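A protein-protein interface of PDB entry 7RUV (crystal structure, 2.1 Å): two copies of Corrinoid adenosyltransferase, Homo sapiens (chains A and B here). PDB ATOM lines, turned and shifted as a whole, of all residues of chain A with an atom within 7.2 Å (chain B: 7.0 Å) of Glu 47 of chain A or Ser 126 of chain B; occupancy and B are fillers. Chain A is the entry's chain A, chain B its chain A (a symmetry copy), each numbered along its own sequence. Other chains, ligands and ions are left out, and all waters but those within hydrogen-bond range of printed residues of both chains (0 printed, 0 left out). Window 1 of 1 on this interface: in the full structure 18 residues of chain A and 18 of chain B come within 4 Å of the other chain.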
ATOM      1  N   SER A  39      21.134  20.872  10.876  1.00  0.00           N
ATOM      2  CA  SER A  39      20.069  21.435  10.047  1.00  0.00           C
ATOM      3  C   SER A  39      20.585  22.571   9.176  1.00  0.00           C
ATOM      4  O   SER A  39      20.162  22.730   8.021  1.00  0.00           O
ATOM      5  CB  SER A  39      18.907  21.922  10.926  1.00  0.00           C
ATOM      6  OG  SER A  39      17.801  22.286  10.120  1.00  0.00           O
ATOM      7  N   SER A  40      21.504  23.361   9.720  1.00  0.00           N
ATOM      8  CA  SER A  40      22.086  24.464   8.973  1.00  0.00           C
ATOM      9  C   SER A  40      22.982  23.956   7.849  1.00  0.00           C
ATOM     10  O   SER A  40      22.911  24.453   6.716  1.00  0.00           O
ATOM     11  CB  SER A  40      22.845  25.380   9.932  1.00  0.00           C
ATOM     12  OG  SER A  40      21.935  25.914  10.890  1.00  0.00           O
ATOM     13  N   ALA A  41      23.816  22.947   8.125  1.00  0.00           N
ATOM     14  CA  ALA A  41      24.582  22.324   7.046  1.00  0.00           C
ATOM     15  C   ALA A  41      23.658  21.826   5.936  1.00  0.00           C
ATOM     16  O   ALA A  41      23.915  22.061   4.744  1.00  0.00           O
ATOM     17  CB  ALA A  41      25.433  21.186   7.600  1.00  0.00           C
ATOM     18  N   ILE A  42      22.547  21.182   6.305  1.00  0.00           N
ATOM     19  CA  ILE A  42      21.612  20.693   5.293  1.00  0.00           C
ATOM     20  C   ILE A  42      20.981  21.857   4.541  1.00  0.00           C
ATOM     21  O   ILE A  42      20.744  21.775   3.326  1.00  0.00           O
ATOM     22  CB  ILE A  42      20.554  19.775   5.941  1.00  0.00           C
ATOM     23  CG1 ILE A  42      21.203  18.440   6.331  1.00  0.00           C
ATOM     24  CG2 ILE A  42      19.352  19.560   4.986  1.00  0.00           C
ATOM     25  CD1 ILE A  42      20.321  17.527   7.158  1.00  0.00           C
ATOM     26  N   GLY A  43      20.710  22.960   5.241  1.00  0.00           N
ATOM     27  CA  GLY A  43      20.237  24.149   4.556  1.00  0.00           C
ATOM     28  C   GLY A  43      21.151  24.580   3.427  1.00  0.00           C
ATOM     29  O   GLY A  43      20.693  24.905   2.329  1.00  0.00           O
ATOM     30  N   PHE A  44      22.460  24.556   3.664  1.00  0.00           N
ATOM     31  CA  PHE A  44      23.371  24.952   2.606  1.00  0.00           C
ATOM     32  C   PHE A  44      23.377  23.926   1.477  1.00  0.00           C
ATOM     33  O   PHE A  44      23.316  24.292   0.296  1.00  0.00           O
ATOM     34  CB  PHE A  44      24.770  25.164   3.175  1.00  0.00           C
ATOM     35  CG  PHE A  44      25.744  25.669   2.169  1.00  0.00           C
ATOM     36  CD1 PHE A  44      26.607  24.792   1.530  1.00  0.00           C
ATOM     37  CD2 PHE A  44      25.800  27.029   1.856  1.00  0.00           C
ATOM     38  CE1 PHE A  44      27.539  25.263   0.585  1.00  0.00           C
ATOM     39  CE2 PHE A  44      26.705  27.509   0.920  1.00  0.00           C
ATOM     40  CZ  PHE A  44      27.586  26.618   0.275  1.00  0.00           C
ATOM     41  N   ALA A  45      23.459  22.630   1.811  1.00  0.00           N
ATOM     42  CA  ALA A  45      23.385  21.608   0.766  1.00  0.00           C
ATOM     43  C   ALA A  45      22.102  21.754  -0.035  1.00  0.00           C
ATOM     44  O   ALA A  45      22.103  21.591  -1.260  1.00  0.00           O
ATOM     45  CB  ALA A  45      23.482  20.201   1.371  1.00  0.00           C
ATOM     46  N   LEU A  46      21.007  22.114   0.640  1.00  0.00           N
ATOM     47  CA  LEU A  46      19.730  22.300  -0.038  1.00  0.00           C
ATOM     48  C   LEU A  46      19.832  23.372  -1.111  1.00  0.00           C
ATOM     49  O   LEU A  46      19.256  23.227  -2.200  1.00  0.00           O
ATOM     50  CB  LEU A  46      18.662  22.662   0.986  1.00  0.00           C
ATOM     51  CG  LEU A  46      17.209  22.432   0.631  1.00  0.00           C
ATOM     52  CD1 LEU A  46      16.507  21.926   1.864  1.00  0.00           C
ATOM     53  CD2 LEU A  46      16.609  23.764   0.165  1.00  0.00           C
ATOM     54  N   GLU A  47      20.588  24.443  -0.830  1.00  0.00           N
ATOM     55  CA  GLU A  47      20.753  25.505  -1.816  1.00  0.00           C
ATOM     56  C   GLU A  47      21.464  24.996  -3.058  1.00  0.00           C
ATOM     57  O   GLU A  47      21.081  25.344  -4.179  1.00  0.00           O
ATOM     58  CB  GLU A  47      21.512  26.692  -1.217  1.00  0.00           C
ATOM     59  CG  GLU A  47      20.822  27.320   0.001  1.00  0.00           C
ATOM     60  CD  GLU A  47      19.412  27.833  -0.299  1.00  0.00           C
ATOM     61  OE1 GLU A  47      18.543  27.762   0.612  1.00  0.00           O
ATOM     62  OE2 GLU A  47      19.179  28.294  -1.447  1.00  0.00           O
ATOM     63  N   LEU A  48      22.497  24.162  -2.885  1.00  0.00           N
ATOM     64  CA  LEU A  48      23.182  23.617  -4.053  1.00  0.00           C
ATOM     65  C   LEU A  48      22.289  22.654  -4.817  1.00  0.00           C
ATOM     66  O   LEU A  48      22.406  22.532  -6.039  1.00  0.00           O
ATOM     67  CB  LEU A  48      24.467  22.912  -3.639  1.00  0.00           C
ATOM     68  CG  LEU A  48      25.403  23.646  -2.691  1.00  0.00           C
ATOM     69  CD1 LEU A  48      26.467  22.681  -2.189  1.00  0.00           C
ATOM     70  CD2 LEU A  48      26.013  24.860  -3.383  1.00  0.00           C
ATOM     71  N   VAL A  49      21.411  21.952  -4.106  1.00  0.00           N
ATOM     72  CA  VAL A  49      20.505  21.007  -4.747  1.00  0.00           C
ATOM     73  C   VAL A  49      19.557  21.753  -5.671  1.00  0.00           C
ATOM     74  O   VAL A  49      19.511  21.501  -6.882  1.00  0.00           O
ATOM     75  CB  VAL A  49      19.740  20.196  -3.684  1.00  0.00           C
ATOM     76  CG1 VAL A  49      18.466  19.598  -4.272  1.00  0.00           C
ATOM     77  CG2 VAL A  49      20.649  19.108  -3.091  1.00  0.00           C
ATOM     78  N   THR A  50      18.828  22.729  -5.107  1.00  0.00           N
ATOM     79  CA  THR A  50      17.800  23.454  -5.850  1.00  0.00           C
ATOM     80  C   THR A  50      18.387  24.220  -7.032  1.00  0.00           C
ATOM     81  O   THR A  50      17.692  24.452  -8.028  1.00  0.00           O
ATOM     82  CB  THR A  50      17.048  24.406  -4.907  1.00  0.00           C
ATOM     83  OG1 THR A  50      17.976  25.278  -4.251  1.00  0.00           O
ATOM     84  CG2 THR A  50      16.307  23.633  -3.836  1.00  0.00           C
ATOM     85  N   GLU A  51      19.661  24.609  -6.953  1.00  0.00           N
ATOM     86  CA  GLU A  51      20.310  25.239  -8.097  1.00  0.00           C
ATOM     87  C   GLU A  51      20.363  24.290  -9.287  1.00  0.00           C
ATOM     88  O   GLU A  51      19.972  24.651 -10.402  1.00  0.00           O
ATOM     89  CB  GLU A  51      21.714  25.701  -7.714  1.00  0.00           C
ATOM     90  CG  GLU A  51      21.746  27.071  -7.073  1.00  0.00           C
ATOM     91  CD  GLU A  51      23.120  27.441  -6.559  1.00  0.00           C
ATOM     92  OE1 GLU A  51      23.235  28.467  -5.855  1.00  0.00           O
ATOM     93  OE2 GLU A  51      24.085  26.701  -6.857  1.00  0.00           O
ATOM     94  N   LYS A  52      20.841  23.069  -9.074  1.00  0.00           N
ATOM     95  CA  LYS A  52      20.865  22.088 -10.151  1.00  0.00           C
ATOM     96  C   LYS A  52      19.542  21.336 -10.304  1.00  0.00           C
ATOM     97  O   LYS A  52      19.505  20.316 -11.001  1.00  0.00           O
ATOM     98  CB  LYS A  52      22.014  21.101  -9.941  1.00  0.00           C
ATOM     99  CG  LYS A  52      23.289  21.536 -10.621  1.00  0.00           C
ATOM    100  CD  LYS A  52      24.426  20.604 -10.292  1.00  0.00           C
ATOM    101  CE  LYS A  52      25.153  20.186 -11.554  1.00  0.00           C
ATOM    102  NZ  LYS A  52      26.463  19.587 -11.219  1.00  0.00           N
ATOM    103  N   GLY A  53      18.474  21.810  -9.660  1.00  0.00           N
ATOM    104  CA  GLY A  53      17.126  21.322  -9.899  1.00  0.00           C
ATOM    105  C   GLY A  53      16.844  19.874  -9.553  1.00  0.00           C
ATOM    106  O   GLY A  53      15.854  19.324 -10.043  1.00  0.00           O
ATOM    107  N   LEU A  60      15.040  16.892   1.769  1.00  0.00           N
ATOM    108  CA  LEU A  60      15.972  17.564   2.679  1.00  0.00           C
ATOM    109  C   LEU A  60      15.242  18.568   3.558  1.00  0.00           C
ATOM    110  O   LEU A  60      15.502  18.651   4.765  1.00  0.00           O
ATOM    111  CB  LEU A  60      17.090  18.259   1.892  1.00  0.00           C
ATOM    112  CG  LEU A  60      18.041  17.283   1.171  1.00  0.00           C
ATOM    113  CD1 LEU A  60      19.008  18.035   0.294  1.00  0.00           C
ATOM    114  CD2 LEU A  60      18.787  16.436   2.176  1.00  0.00           C
ATOM    115  N   GLN A  64      14.628  18.834   7.692  1.00  0.00           N
ATOM    116  CA  GLN A  64      14.845  19.994   8.561  1.00  0.00           C
ATOM    117  C   GLN A  64      13.686  20.162   9.532  1.00  0.00           C
ATOM    118  O   GLN A  64      13.894  20.508  10.704  1.00  0.00           O
ATOM    119  CB  GLN A  64      15.021  21.264   7.731  1.00  0.00           C
ATOM    120  CG  GLN A  64      16.388  21.354   7.055  1.00  0.00           C
ATOM    121  CD  GLN A  64      16.545  22.643   6.290  1.00  0.00           C
ATOM    122  OE1 GLN A  64      15.734  22.968   5.414  1.00  0.00           O
ATOM    123  NE2 GLN A  64      17.570  23.399   6.629  1.00  0.00           N
ATOM    124  N   ILE A 124      27.205  18.891  -4.778  1.00  0.00           N
ATOM    125  CA  ILE A 124      26.087  18.424  -3.962  1.00  0.00           C
ATOM    126  C   ILE A 124      26.487  17.196  -3.154  1.00  0.00           C
ATOM    127  O   ILE A 124      26.287  17.145  -1.935  1.00  0.00           O
ATOM    128  CB  ILE A 124      24.862  18.128  -4.846  1.00  0.00           C
ATOM    129  CG1 ILE A 124      24.209  19.431  -5.303  1.00  0.00           C
ATOM    130  CG2 ILE A 124      23.842  17.277  -4.090  1.00  0.00           C
ATOM    131  CD1 ILE A 124      23.379  19.276  -6.581  1.00  0.00           C
ATOM    132  N   LEU B  48      30.932  34.284  -0.428  1.00  0.00           N
ATOM    133  CA  LEU B  48      29.639  34.277  -1.106  1.00  0.00           C
ATOM    134  C   LEU B  48      28.979  35.645  -1.049  1.00  0.00           C
ATOM    135  O   LEU B  48      28.238  36.016  -1.963  1.00  0.00           O
ATOM    136  CB  LEU B  48      28.717  33.234  -0.487  1.00  0.00           C
ATOM    137  CG  LEU B  48      29.279  31.838  -0.264  1.00  0.00           C
ATOM    138  CD1 LEU B  48      28.313  31.042   0.602  1.00  0.00           C
ATOM    139  CD2 LEU B  48      29.544  31.154  -1.601  1.00  0.00           C
ATOM    140  N   PRO B 119      16.627  26.770   8.507  1.00  0.00           N
ATOM    141  CA  PRO B 119      17.812  27.534   8.073  1.00  0.00           C
ATOM    142  C   PRO B 119      17.891  27.806   6.558  1.00  0.00           C
ATOM    143  O   PRO B 119      18.063  26.794   5.899  1.00  0.00           O
ATOM    144  CB  PRO B 119      18.966  26.638   8.511  1.00  0.00           C
ATOM    145  CG  PRO B 119      18.426  25.956   9.770  1.00  0.00           C
ATOM    146  CD  PRO B 119      16.966  25.681   9.443  1.00  0.00           C
ATOM    147  N   GLY B 121      17.626  30.044   3.474  1.00  0.00           N
ATOM    148  CA  GLY B 121      16.950  31.009   2.598  1.00  0.00           C
ATOM    149  C   GLY B 121      17.855  31.673   1.549  1.00  0.00           C
ATOM    150  O   GLY B 121      17.929  32.898   1.444  1.00  0.00           O
ATOM    151  N   GLY B 122      18.535  30.859   0.754  1.00  0.00           N
ATOM    152  CA  GLY B 122      19.577  31.344  -0.126  1.00  0.00           C
ATOM    153  C   GLY B 122      20.954  30.878   0.335  1.00  0.00           C
ATOM    154  O   GLY B 122      21.154  30.454   1.477  1.00  0.00           O
ATOM    155  N   LYS B 123      21.921  30.948  -0.584  1.00  0.00           N
ATOM    156  CA  LYS B 123      23.250  30.421  -0.277  1.00  0.00           C
ATOM    157  C   LYS B 123      23.920  31.220   0.837  1.00  0.00           C
ATOM    158  O   LYS B 123      24.461  30.643   1.791  1.00  0.00           O
ATOM    159  CB  LYS B 123      24.130  30.411  -1.529  1.00  0.00           C
ATOM    160  CG  LYS B 123      24.518  29.021  -1.993  1.00  0.00           C
ATOM    161  CD  LYS B 123      25.783  29.033  -2.834  1.00  0.00           C
ATOM    162  CE  LYS B 123      25.543  29.672  -4.183  1.00  0.00           C
ATOM    163  NZ  LYS B 123      26.570  29.178  -5.144  1.00  0.00           N
ATOM    164  N   ILE B 124      23.917  32.550   0.719  1.00  0.00           N
ATOM    165  CA  ILE B 124      24.499  33.391   1.761  1.00  0.00           C
ATOM    166  C   ILE B 124      23.803  33.153   3.096  1.00  0.00           C
ATOM    167  O   ILE B 124      24.456  32.911   4.118  1.00  0.00           O
ATOM    168  CB  ILE B 124      24.428  34.875   1.359  1.00  0.00           C
ATOM    169  CG1 ILE B 124      25.469  35.186   0.285  1.00  0.00           C
ATOM    170  CG2 ILE B 124      24.652  35.776   2.572  1.00  0.00           C
ATOM    171  CD1 ILE B 124      25.123  36.417  -0.556  1.00  0.00           C
ATOM    172  N   SER B 125      22.468  33.240   3.113  1.00  0.00           N
ATOM    173  CA  SER B 125      21.737  33.060   4.365  1.00  0.00           C
ATOM    174  C   SER B 125      22.027  31.696   4.997  1.00  0.00           C
ATOM    175  O   SER B 125      22.291  31.600   6.201  1.00  0.00           O
ATOM    176  CB  SER B 125      20.238  33.226   4.127  1.00  0.00           C
ATOM    177  OG  SER B 125      19.536  32.876   5.303  1.00  0.00           O
ATOM    178  N   SER B 126      21.973  30.610   4.210  1.00  0.00           N
ATOM    179  CA  SER B 126      22.220  29.294   4.799  1.00  0.00           C
ATOM    180  C   SER B 126      23.653  29.182   5.298  1.00  0.00           C
ATOM    181  O   SER B 126      23.896  28.598   6.360  1.00  0.00           O
ATOM    182  CB  SER B 126      21.899  28.180   3.794  1.00  0.00           C
ATOM    183  OG  SER B 126      22.733  28.288   2.656  1.00  0.00           O
ATOM    184  N   ALA B 127      24.608  29.772   4.576  1.00  0.00           N
ATOM    185  CA  ALA B 127      25.989  29.778   5.054  1.00  0.00           C
ATOM    186  C   ALA B 127      26.103  30.508   6.378  1.00  0.00           C
ATOM    187  O   ALA B 127      26.824  30.056   7.283  1.00  0.00           O
ATOM    188  CB  ALA B 127      26.913  30.414   4.021  1.00  0.00           C
ATOM    189  N   LEU B 128      25.387  31.642   6.516  1.00  0.00           N
ATOM    190  CA  LEU B 128      25.400  32.384   7.772  1.00  0.00           C
ATOM    191  C   LEU B 128      24.741  31.597   8.897  1.00  0.00           C
ATOM    192  O   LEU B 128      25.198  31.672  10.047  1.00  0.00           O
ATOM    193  CB  LEU B 128      24.724  33.753   7.593  1.00  0.00           C
ATOM    194  CG  LEU B 128      25.531  34.731   6.723  1.00  0.00           C
ATOM    195  CD1 LEU B 128      24.748  35.977   6.351  1.00  0.00           C
ATOM    196  CD2 LEU B 128      26.863  35.082   7.395  1.00  0.00           C
ATOM    197  N   HIS B 129      23.681  30.824   8.592  1.00  0.00           N
ATOM    198  CA  HIS B 129      23.093  29.972   9.620  1.00  0.00           C
ATOM    199  C   HIS B 129      24.089  28.922  10.084  1.00  0.00           C
ATOM    200  O   HIS B 129      24.165  28.618  11.281  1.00  0.00           O
ATOM    201  CB  HIS B 129      21.801  29.316   9.115  1.00  0.00           C
ATOM    202  CG  HIS B 129      20.616  30.219   9.194  1.00  0.00           C
ATOM    203  ND1 HIS B 129      20.224  30.817  10.372  1.00  0.00           N
ATOM    204  CD2 HIS B 129      19.761  30.663   8.242  1.00  0.00           C
ATOM    205  CE1 HIS B 129      19.166  31.575  10.144  1.00  0.00           C
ATOM    206  NE2 HIS B 129      18.870  31.505   8.860  1.00  0.00           N
ATOM    207  N   PHE B 130      24.885  28.375   9.162  1.00  0.00           N
ATOM    208  CA  PHE B 130      25.929  27.444   9.584  1.00  0.00           C
ATOM    209  C   PHE B 130      26.984  28.147  10.441  1.00  0.00           C
ATOM    210  O   PHE B 130      27.402  27.610  11.477  1.00  0.00           O
ATOM    211  CB  PHE B 130      26.575  26.759   8.374  1.00  0.00           C
ATOM    212  CG  PHE B 130      27.674  25.785   8.756  1.00  0.00           C
ATOM    213  CD1 PHE B 130      27.367  24.551   9.325  1.00  0.00           C
ATOM    214  CD2 PHE B 130      29.015  26.113   8.557  1.00  0.00           C
ATOM    215  CE1 PHE B 130      28.393  23.653   9.677  1.00  0.00           C
ATOM    216  CE2 PHE B 130      30.041  25.223   8.917  1.00  0.00           C
ATOM    217  CZ  PHE B 130      29.726  24.000   9.480  1.00  0.00           C
ATOM    218  N   CYS B 131      27.409  29.356  10.040  1.00  0.00           N
ATOM    219  CA  CYS B 131      28.304  30.156  10.883  1.00  0.00           C
ATOM    220  C   CYS B 131      27.711  30.398  12.272  1.00  0.00           C
ATOM    221  O   CYS B 131      28.422  30.301  13.285  1.00  0.00           O
ATOM    222  CB  CYS B 131      28.600  31.489  10.195  1.00  0.00           C
ATOM    223  SG  CYS B 131      29.636  31.362   8.786  1.00  0.00           S
ATOM    224  N   ARG B 132      26.395  30.650  12.321  1.00  0.00           N
ATOM    225  CA  ARG B 132      25.688  30.878  13.582  1.00  0.00           C
ATOM    226  C   ARG B 132      25.795  29.665  14.511  1.00  0.00           C
ATOM    227  O   ARG B 132      26.092  29.794  15.709  1.00  0.00           O
ATOM    228  CB  ARG B 132      24.219  31.203  13.276  1.00  0.00           C
ATOM    229  CG  ARG B 132      23.293  31.436  14.461  1.00  0.00           C
ATOM    230  CD  ARG B 132      21.797  31.510  14.021  1.00  0.00           C
ATOM    231  NE  ARG B 132      21.445  30.313  13.265  1.00  0.00           N
ATOM    232  CZ  ARG B 132      21.207  29.142  13.840  1.00  0.00           C
ATOM    233  NH1 ARG B 132      20.965  28.069  13.098  1.00  0.00           N
ATOM    234  NH2 ARG B 132      21.230  29.055  15.168  1.00  0.00           N
ATOM    235  N   ALA B 170      21.434  36.640   8.518  1.00  0.00           N
ATOM    236  CA  ALA B 170      20.936  35.645   7.578  1.00  0.00           C
ATOM    237  C   ALA B 170      19.495  35.954   7.164  1.00  0.00           C
ATOM    238  O   ALA B 170      19.158  35.910   5.974  1.00  0.00           O
ATOM    239  CB  ALA B 170      21.055  34.250   8.190  1.00  0.00           C
ATOM    240  N   ALA B 174      18.406  36.888   3.332  1.00  0.00           N
ATOM    241  CA  ALA B 174      17.307  36.166   2.690  1.00  0.00           C
ATOM    242  C   ALA B 174      16.215  37.125   2.226  1.00  0.00           C
ATOM    243  O   ALA B 174      15.724  37.010   1.097  1.00  0.00           O
ATOM    244  CB  ALA B 174      16.724  35.111   3.634  1.00  0.00           C
ATOM    245  N   GLU B 177      17.158  39.115  -0.798  1.00  0.00           N
ATOM    246  CA  GLU B 177      17.163  38.301  -2.005  1.00  0.00           C
ATOM    247  C   GLU B 177      15.767  37.919  -2.462  1.00  0.00           C
ATOM    248  O   GLU B 177      15.633  37.273  -3.507  1.00  0.00           O
ATOM    249  CB  GLU B 177      18.006  37.036  -1.796  1.00  0.00           C
ATOM    250  CG  GLU B 177      19.506  37.348  -1.663  1.00  0.00           C
ATOM    251  CD  GLU B 177      20.374  36.096  -1.587  1.00  0.00           C
ATOM    252  OE1 GLU B 177      21.590  36.239  -1.324  1.00  0.00           O
ATOM    253  OE2 GLU B 177      19.848  34.981  -1.796  1.00  0.00           O
ATOM    254  N   ASN B 179      13.774  35.824  -0.939  1.00  0.00           N
ATOM    255  CA  ASN B 179      13.470  34.463  -0.516  1.00  0.00           C
ATOM    256  C   ASN B 179      12.567  34.502   0.700  1.00  0.00           C
ATOM    257  O   ASN B 179      12.794  35.278   1.634  1.00  0.00           O
ATOM    258  CB  ASN B 179      14.757  33.698  -0.198  1.00  0.00           C
ATOM    259  CG  ASN B 179      15.663  33.585  -1.390  1.00  0.00           C
ATOM    260  OD1 ASN B 179      15.190  33.535  -2.524  1.00  0.00           O
ATOM    261  ND2 ASN B 179      16.964  33.559  -1.156  1.00  0.00           N
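OE1 of Glu 51 of chain A lies within salt-bridge range of NZ of Lys 123 of chain B. The side-chain hydroxyl (OG) of Ser 40 of chain A sits at hydrogen-bond distance from the guanidinium group (NH1) of Arg 132 of chain B (3.2 Å). OE1 of Glu 47 of chain A lies within hydrogen-bond range of N of Gly 122 of chain B (3.1 Å).
The side-chain amide nitrogen (NE2) of Gln 64 of chain A sits at hydrogen-bond distance from the backbone carbonyl oxygen (O) of Ser 39 of chain A (3.0 Å). The backbone carbonyl oxygen of Glu 47 of chain A sits at hydrogen-bond distance from the side-chain hydroxyl of Thr 50 of chain A, 3.1 Å away. O of Gly 121 of chain B lies within hydrogen-bond range of ND2 of Asn 179 of chain B (2.9 Å). OG of Ser 126 of chain B is in hydrogen-bond range of O of Gly 122 of chain B (2.9 Å). The side-chain amide nitrogen of Gln 64 of chain A lies close to the backbone NH of Gly 43 of chain A, at 3.5 Å. O of Lys 123 of chain B is in hydrogen-bond range of OG of Ser 126 of chain B (3.0 Å).
Pro 119 of chain B touches Ser 39 of chain A (CD to OG, 3.6 Å). Ser 40 of chain A touches Pro 119 of chain B (OG to CG, 3.7 Å). OG of Ser 40 of chain A touches O of His 129 of chain B, 3.5 Å away. C of Gly 43 of chain A touches CB of Ser 126 of chain B (3.7 Å). CE2 of Phe 44 of chain A touches CD1 of Leu 48 of chain B, at 3.9 Å. Lys 123 of chain B touches Phe 44 of chain A (O to CD2, 3.9 Å). N of Gly 121 of chain B touches OE1 of Glu 47 of chain A, 3.8 Å away. Lys 123 of chain B touches Glu 47 of chain A. Glu 47 of chain A touches Ser 126 of chain B (CG to OG, 3.4 Å). Gln 64 of chain A touches Pro 119 of chain B.
Of the printed residues of chain B, Glu 47 of chain A touches Gly 121 (3.8 Å), Gly 122 (3.1 Å), Lys 123 (3.8 Å) and Ser 126 (3.4 Å). Ser 126 of chain B touches just these residues of chain A: Gly 43, Phe 44 and Glu 47. Printed residues of chain B within 4 Å of Ser 39 of chain A: Pro 119 (3.6 Å). Of the printed residues of chain B, Gln 64 of chain A touches Pro 119 (3.5 Å). Of the printed residues of chain A, His 129 of chain B touches Ser 40 (3.5 Å). Ile 124 of chain B touches none of the printed residues of chain A. Leu 60 of chain A touches none of the printed residues of chain B. The nearest printed residue of chain B that does not touch Ser 39 of chain A is Arg 132 of chain B (6.8 Å).
Of the 18 printed residues of chain A, 7 touch a printed residue of chain B. Among the printed residues, Asp or Glu carboxylates within 4 Å of a Lys or Arg side-chain nitrogen of the other chain: Glu 51 of chain A with Lys 123 of chain B (3.5 Å).
Positions printed for both chains: 48 and 124. Of the 16 pairs that touch across the chains among the printed residues, none has its exchanged pair printed and touching as well.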
